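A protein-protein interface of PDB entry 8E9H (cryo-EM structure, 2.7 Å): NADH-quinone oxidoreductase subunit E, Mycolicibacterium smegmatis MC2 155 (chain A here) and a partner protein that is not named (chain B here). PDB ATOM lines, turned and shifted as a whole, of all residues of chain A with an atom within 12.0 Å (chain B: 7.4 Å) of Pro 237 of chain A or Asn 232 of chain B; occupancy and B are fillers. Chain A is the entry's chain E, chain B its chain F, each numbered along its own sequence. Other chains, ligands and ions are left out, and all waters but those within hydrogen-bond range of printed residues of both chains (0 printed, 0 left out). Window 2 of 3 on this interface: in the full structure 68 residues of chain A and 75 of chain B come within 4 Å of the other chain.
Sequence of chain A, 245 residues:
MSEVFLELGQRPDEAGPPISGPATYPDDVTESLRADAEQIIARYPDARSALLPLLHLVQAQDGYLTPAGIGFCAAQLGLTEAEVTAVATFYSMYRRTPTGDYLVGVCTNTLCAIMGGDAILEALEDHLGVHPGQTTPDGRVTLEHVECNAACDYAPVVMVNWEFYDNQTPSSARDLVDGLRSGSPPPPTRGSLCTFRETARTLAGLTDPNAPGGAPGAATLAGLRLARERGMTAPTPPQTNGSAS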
ATOM      1  N   THR A 233      13.163 -19.633   2.405  1.00  0.00           N
ATOM      2  CA  THR A 233      13.848 -18.367   2.192  1.00  0.00           C
ATOM      3  C   THR A 233      15.269 -18.640   1.725  1.00  0.00           C
ATOM      4  O   THR A 233      15.721 -19.785   1.663  1.00  0.00           O
ATOM      5  CB  THR A 233      13.875 -17.512   3.465  1.00  0.00           C
ATOM      6  OG1 THR A 233      14.630 -18.183   4.480  1.00  0.00           O
ATOM      7  CG2 THR A 233      12.467 -17.254   3.973  1.00  0.00           C
ATOM      8  N   ALA A 234      15.973 -17.563   1.395  1.00  0.00           N
ATOM      9  CA  ALA A 234      17.367 -17.649   0.989  1.00  0.00           C
ATOM     10  C   ALA A 234      18.219 -18.053   2.185  1.00  0.00           C
ATOM     11  O   ALA A 234      17.822 -17.823   3.333  1.00  0.00           O
ATOM     12  CB  ALA A 234      17.843 -16.314   0.416  1.00  0.00           C
ATOM     13  N   PRO A 235      19.388 -18.660   1.966  1.00  0.00           N
ATOM     14  CA  PRO A 235      20.216 -19.097   3.098  1.00  0.00           C
ATOM     15  C   PRO A 235      20.794 -17.963   3.927  1.00  0.00           C
ATOM     16  O   PRO A 235      21.307 -18.228   5.023  1.00  0.00           O
ATOM     17  CB  PRO A 235      21.330 -19.904   2.420  1.00  0.00           C
ATOM     18  CG  PRO A 235      21.428 -19.334   1.059  1.00  0.00           C
ATOM     19  CD  PRO A 235      20.031 -18.945   0.673  1.00  0.00           C
ATOM     20  N   THR A 236      20.739 -16.722   3.451  1.00  0.00           N
ATOM     21  CA  THR A 236      21.260 -15.580   4.193  1.00  0.00           C
ATOM     22  C   THR A 236      22.781 -15.661   4.278  1.00  0.00           C
ATOM     23  O   THR A 236      23.340 -16.765   4.310  1.00  0.00           O
ATOM     24  CB  THR A 236      20.666 -15.520   5.601  1.00  0.00           C
ATOM     25  OG1 THR A 236      21.113 -16.648   6.364  1.00  0.00           O
ATOM     26  CG2 THR A 236      19.149 -15.524   5.542  1.00  0.00           C
ATOM     27  N   PRO A 237      23.489 -14.522   4.317  1.00  0.00           N
ATOM     28  CA  PRO A 237      24.956 -14.524   4.368  1.00  0.00           C
ATOM     29  C   PRO A 237      25.522 -15.429   5.457  1.00  0.00           C
ATOM     30  O   PRO A 237      26.735 -15.415   5.666  1.00  0.00           O
ATOM     31  CB  PRO A 237      25.298 -13.061   4.656  1.00  0.00           C
ATOM     32  CG  PRO A 237      24.153 -12.294   4.120  1.00  0.00           C
ATOM     33  CD  PRO A 237      22.944 -13.153   4.330  1.00  0.00           C
ATOM     34  N   VAL B   7      15.014 -14.795  -4.143  1.00  0.00           N
ATOM     35  CA  VAL B   7      16.052 -13.775  -4.056  1.00  0.00           C
ATOM     36  C   VAL B   7      15.655 -12.621  -4.962  1.00  0.00           C
ATOM     37  O   VAL B   7      15.457 -11.492  -4.501  1.00  0.00           O
ATOM     38  CB  VAL B   7      17.426 -14.344  -4.447  1.00  0.00           C
ATOM     39  CG1 VAL B   7      18.473 -13.246  -4.447  1.00  0.00           C
ATOM     40  CG2 VAL B   7      17.819 -15.462  -3.503  1.00  0.00           C
ATOM     41  N   ARG B  10      12.053 -12.104  -4.310  1.00  0.00           N
ATOM     42  CA  ARG B  10      11.839 -11.709  -2.924  1.00  0.00           C
ATOM     43  C   ARG B  10      10.964 -10.467  -2.798  1.00  0.00           C
ATOM     44  O   ARG B  10      10.028 -10.432  -1.993  1.00  0.00           O
ATOM     45  CB  ARG B  10      13.204 -11.482  -2.273  1.00  0.00           C
ATOM     46  CG  ARG B  10      13.196 -10.677  -0.984  1.00  0.00           C
ATOM     47  CD  ARG B  10      14.611 -10.434  -0.465  1.00  0.00           C
ATOM     48  NE  ARG B  10      15.567 -10.145  -1.531  1.00  0.00           N
ATOM     49  CZ  ARG B  10      16.819  -9.765  -1.326  1.00  0.00           C
ATOM     50  NH1 ARG B  10      17.308  -9.618  -0.105  1.00  0.00           N
ATOM     51  NH2 ARG B  10      17.602  -9.523  -2.373  1.00  0.00           N
ATOM     52  N   ASP B  27      18.127  -3.135   0.162  1.00  0.00           N
ATOM     53  CA  ASP B  27      19.557  -3.175  -0.130  1.00  0.00           C
ATOM     54  C   ASP B  27      19.850  -2.938  -1.604  1.00  0.00           C
ATOM     55  O   ASP B  27      20.942  -3.255  -2.081  1.00  0.00           O
ATOM     56  CB  ASP B  27      20.173  -4.506   0.316  1.00  0.00           C
ATOM     57  N   PHE B  46      35.671 -11.666  -8.780  1.00  0.00           N
ATOM     58  CA  PHE B  46      34.622 -11.944  -7.809  1.00  0.00           C
ATOM     59  C   PHE B  46      33.502 -12.747  -8.448  1.00  0.00           C
ATOM     60  O   PHE B  46      33.000 -13.715  -7.865  1.00  0.00           O
ATOM     61  CB  PHE B  46      34.095 -10.623  -7.248  1.00  0.00           C
ATOM     62  CG  PHE B  46      33.052 -10.780  -6.184  1.00  0.00           C
ATOM     63  CD1 PHE B  46      31.720 -10.938  -6.518  1.00  0.00           C
ATOM     64  CD2 PHE B  46      33.402 -10.745  -4.847  1.00  0.00           C
ATOM     65  CE1 PHE B  46      30.759 -11.075  -5.538  1.00  0.00           C
ATOM     66  CE2 PHE B  46      32.446 -10.879  -3.863  1.00  0.00           C
ATOM     67  CZ  PHE B  46      31.122 -11.043  -4.209  1.00  0.00           C
ATOM     68  N   PRO B 227      23.935  -8.524  -8.790  1.00  0.00           N
ATOM     69  CA  PRO B 227      23.808  -7.718  -7.573  1.00  0.00           C
ATOM     70  C   PRO B 227      23.537  -8.571  -6.346  1.00  0.00           C
ATOM     71  O   PRO B 227      24.092  -8.302  -5.271  1.00  0.00           O
ATOM     72  CB  PRO B 227      22.636  -6.772  -7.887  1.00  0.00           C
ATOM     73  CG  PRO B 227      22.084  -7.206  -9.215  1.00  0.00           C
ATOM     74  CD  PRO B 227      23.162  -7.954  -9.902  1.00  0.00           C
ATOM     75  N   PRO B 228      22.710  -9.616  -6.452  1.00  0.00           N
ATOM     76  CA  PRO B 228      22.540 -10.524  -5.309  1.00  0.00           C
ATOM     77  C   PRO B 228      23.830 -11.139  -4.809  1.00  0.00           C
ATOM     78  O   PRO B 228      23.921 -11.423  -3.610  1.00  0.00           O
ATOM     79  CB  PRO B 228      21.597 -11.597  -5.857  1.00  0.00           C
ATOM     80  CG  PRO B 228      20.773 -10.883  -6.830  1.00  0.00           C
ATOM     81  CD  PRO B 228      21.633  -9.803  -7.434  1.00  0.00           C
ATOM     82  N   ILE B 229      24.819 -11.365  -5.669  1.00  0.00           N
ATOM     83  CA  ILE B 229      26.068 -11.971  -5.224  1.00  0.00           C
ATOM     84  C   ILE B 229      27.108 -10.932  -4.826  1.00  0.00           C
ATOM     85  O   ILE B 229      27.984 -11.238  -4.004  1.00  0.00           O
ATOM     86  CB  ILE B 229      26.649 -12.912  -6.297  1.00  0.00           C
ATOM     87  CG1 ILE B 229      26.994 -12.156  -7.575  1.00  0.00           C
ATOM     88  CG2 ILE B 229      25.653 -13.986  -6.632  1.00  0.00           C
ATOM     89  CD1 ILE B 229      27.850 -12.954  -8.521  1.00  0.00           C
ATOM     90  N   MET B 230      27.044  -9.720  -5.376  1.00  0.00           N
ATOM     91  CA  MET B 230      27.954  -8.677  -4.922  1.00  0.00           C
ATOM     92  C   MET B 230      27.705  -8.357  -3.457  1.00  0.00           C
ATOM     93  O   MET B 230      28.648  -8.177  -2.679  1.00  0.00           O
ATOM     94  CB  MET B 230      27.812  -7.432  -5.790  1.00  0.00           C
ATOM     95  CG  MET B 230      28.248  -7.660  -7.222  1.00  0.00           C
ATOM     96  SD  MET B 230      29.982  -8.142  -7.340  1.00  0.00           S
ATOM     97  CE  MET B 230      30.800  -6.629  -6.861  1.00  0.00           C
ATOM     98  N   VAL B 231      26.434  -8.278  -3.060  1.00  0.00           N
ATOM     99  CA  VAL B 231      26.111  -8.427  -1.652  1.00  0.00           C
ATOM    100  C   VAL B 231      25.980  -9.912  -1.333  1.00  0.00           C
ATOM    101  O   VAL B 231      25.864 -10.762  -2.221  1.00  0.00           O
ATOM    102  CB  VAL B 231      24.832  -7.661  -1.279  1.00  0.00           C
ATOM    103  CG1 VAL B 231      25.044  -6.170  -1.459  1.00  0.00           C
ATOM    104  CG2 VAL B 231      23.650  -8.133  -2.107  1.00  0.00           C
ATOM    105  N   ASN B 232      26.046 -10.229  -0.044  1.00  0.00           N
ATOM    106  CA  ASN B 232      25.927 -11.606   0.426  1.00  0.00           C
ATOM    107  C   ASN B 232      27.188 -12.410   0.126  1.00  0.00           C
ATOM    108  O   ASN B 232      27.321 -13.548   0.583  1.00  0.00           O
ATOM    109  CB  ASN B 232      24.715 -12.293  -0.209  1.00  0.00           C
ATOM    110  CG  ASN B 232      23.442 -11.500  -0.037  1.00  0.00           C
ATOM    111  OD1 ASN B 232      23.208 -10.900   1.010  1.00  0.00           O
ATOM    112  ND2 ASN B 232      22.610 -11.489  -1.068  1.00  0.00           N
ATOM    113  N   GLY B 233      28.123 -11.835  -0.625  1.00  0.00           N
ATOM    114  CA  GLY B 233      29.388 -12.481  -0.895  1.00  0.00           C
ATOM    115  C   GLY B 233      29.266 -13.655  -1.850  1.00  0.00           C
ATOM    116  O   GLY B 233      28.189 -14.012  -2.330  1.00  0.00           O
ATOM    117  N   VAL B 234      30.419 -14.270  -2.120  1.00  0.00           N
ATOM    118  CA  VAL B 234      30.469 -15.408  -3.036  1.00  0.00           C
ATOM    119  C   VAL B 234      29.969 -16.668  -2.344  1.00  0.00           C
ATOM    120  O   VAL B 234      29.182 -17.439  -2.906  1.00  0.00           O
ATOM    121  CB  VAL B 234      31.898 -15.601  -3.571  1.00  0.00           C
ATOM    122  CG1 VAL B 234      32.063 -16.992  -4.160  1.00  0.00           C
ATOM    123  CG2 VAL B 234      32.225 -14.538  -4.602  1.00  0.00           C
ATOM    124  N   ASP B 235      30.427 -16.899  -1.112  1.00  0.00           N
ATOM    125  CA  ASP B 235      30.086 -18.134  -0.417  1.00  0.00           C
ATOM    126  C   ASP B 235      28.580 -18.318  -0.307  1.00  0.00           C
ATOM    127  O   ASP B 235      28.084 -19.446  -0.388  1.00  0.00           O
ATOM    128  CB  ASP B 235      30.723 -18.146   0.972  1.00  0.00           C
ATOM    129  N   TRP B 236      27.838 -17.226  -0.130  1.00  0.00           N
ATOM    130  CA  TRP B 236      26.385 -17.330  -0.070  1.00  0.00           C
ATOM    131  C   TRP B 236      25.828 -17.905  -1.363  1.00  0.00           C
ATOM    132  O   TRP B 236      24.980 -18.804  -1.342  1.00  0.00           O
ATOM    133  CB  TRP B 236      25.785 -15.956   0.212  1.00  0.00           C
ATOM    134  CG  TRP B 236      24.319 -15.883   0.006  1.00  0.00           C
ATOM    135  CD1 TRP B 236      23.350 -16.161   0.919  1.00  0.00           C
ATOM    136  CD2 TRP B 236      23.644 -15.494  -1.192  1.00  0.00           C
ATOM    137  NE1 TRP B 236      22.109 -15.973   0.364  1.00  0.00           N
ATOM    138  CE2 TRP B 236      22.263 -15.563  -0.933  1.00  0.00           C
ATOM    139  CE3 TRP B 236      24.073 -15.095  -2.459  1.00  0.00           C
ATOM    140  CZ2 TRP B 236      21.309 -15.250  -1.894  1.00  0.00           C
ATOM    141  CZ3 TRP B 236      23.125 -14.785  -3.411  1.00  0.00           C
ATOM    142  CH2 TRP B 236      21.760 -14.864  -3.125  1.00  0.00           C
ATOM    143  N   PHE B 237      26.300 -17.401  -2.504  1.00  0.00           N
ATOM    144  CA  PHE B 237      25.865 -17.938  -3.788  1.00  0.00           C
ATOM    145  C   PHE B 237      26.279 -19.393  -3.945  1.00  0.00           C
ATOM    146  O   PHE B 237      25.473 -20.233  -4.360  1.00  0.00           O
ATOM    147  CB  PHE B 237      26.444 -17.087  -4.917  1.00  0.00           C
ATOM    148  CG  PHE B 237      25.872 -17.391  -6.270  1.00  0.00           C
ATOM    149  CD1 PHE B 237      24.634 -16.906  -6.644  1.00  0.00           C
ATOM    150  CD2 PHE B 237      26.593 -18.138  -7.182  1.00  0.00           C
ATOM    151  CE1 PHE B 237      24.119 -17.174  -7.894  1.00  0.00           C
ATOM    152  CE2 PHE B 237      26.083 -18.408  -8.430  1.00  0.00           C
ATOM    153  CZ  PHE B 237      24.849 -17.920  -8.789  1.00  0.00           C
ATOM    154  N   MET B 240      24.246 -22.564  -2.681  1.00  0.00           N
ATOM    155  CA  MET B 240      23.078 -23.082  -3.374  1.00  0.00           C
ATOM    156  C   MET B 240      23.510 -23.838  -4.621  1.00  0.00           C
ATOM    157  O   MET B 240      24.403 -23.395  -5.349  1.00  0.00           O
ATOM    158  CB  MET B 240      22.131 -21.946  -3.755  1.00  0.00           C
ATOM    159  CG  MET B 240      21.837 -21.000  -2.613  1.00  0.00           C
ATOM    160  SD  MET B 240      20.531 -19.834  -3.014  1.00  0.00           S
ATOM    161  CE  MET B 240      21.494 -18.347  -3.263  1.00  0.00           C
ATOM    162  N   PHE B 248      21.107 -19.827  -7.484  1.00  0.00           N
ATOM    163  CA  PHE B 248      19.664 -19.871  -7.636  1.00  0.00           C
ATOM    164  C   PHE B 248      19.284 -19.532  -9.069  1.00  0.00           C
ATOM    165  O   PHE B 248      20.041 -18.896  -9.804  1.00  0.00           O
ATOM    166  CB  PHE B 248      19.003 -18.886  -6.680  1.00  0.00           C
ATOM    167  CG  PHE B 248      19.397 -17.462  -6.927  1.00  0.00           C
ATOM    168  CD1 PHE B 248      20.543 -16.938  -6.357  1.00  0.00           C
ATOM    169  CD2 PHE B 248      18.625 -16.649  -7.732  1.00  0.00           C
ATOM    170  CE1 PHE B 248      20.910 -15.634  -6.589  1.00  0.00           C
ATOM    171  CE2 PHE B 248      18.988 -15.342  -7.964  1.00  0.00           C
ATOM    172  CZ  PHE B 248      20.130 -14.834  -7.391  1.00  0.00           C
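Of the printed residues of chain B, Pro 235 of chain A touches Trp 236 (3.5 Å) and Met 240 (3.8 Å).
Of the printed residues of chain B, Thr 236 of chain A touches Trp 236.
Pro 237 of chain A touches two residues of chain B.
Val 231 of chain B touches none of the printed residues of chain A.
Asn 232 of chain B touches just one residue of chain A: Pro 237.
No residue of chain A comes within 4 Å of Gly 233 of chain B.
No residue of chain A comes within 4 Å of Val 234 of chain B.
Trp 236 of chain B touches just these residues of chain A: Pro 235, Thr 236 and Pro 237.
Of the printed residues of chain A, Met 240 of chain B touches Pro 235.
The nearest residue of chain A that does not touch Asn 232 of chain B is Thr 236 of chain A (5.8 Å).
The nearest printed residue of chain A that does not touch Met 240 of chain B is Ala 234 of chain A (5.6 Å).
CG of Pro 235 of chain A touches NE1 of Trp 236 of chain B, 3.5 Å away.
Met 240 of chain B touches Pro 235 of chain A.
Asn 232 of chain B touches Pro 237 of chain A.
CD1 of Trp 236 of chain B touches N of Pro 237 of chain A, at 3.8 Å.
O of Pro 228 of chain B is in hydrogen-bond range of ND2 of Asn 232 of chain B.
The indole nitrogen (NE1) of Trp 236 of chain B lies close to the backbone NH (N) of Thr 236 of chain A (3.5 Å).
Hydrophobic or aromatic side chains of chain B that line the printed part of chain A: Trp 236 and Met 240.
Of the 5 printed residues of chain A, 3 touch a printed residue of chain B.
Hydrophobic or aromatic side chains of chain A that line the printed part of chain B: Pro 235 and Pro 237.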
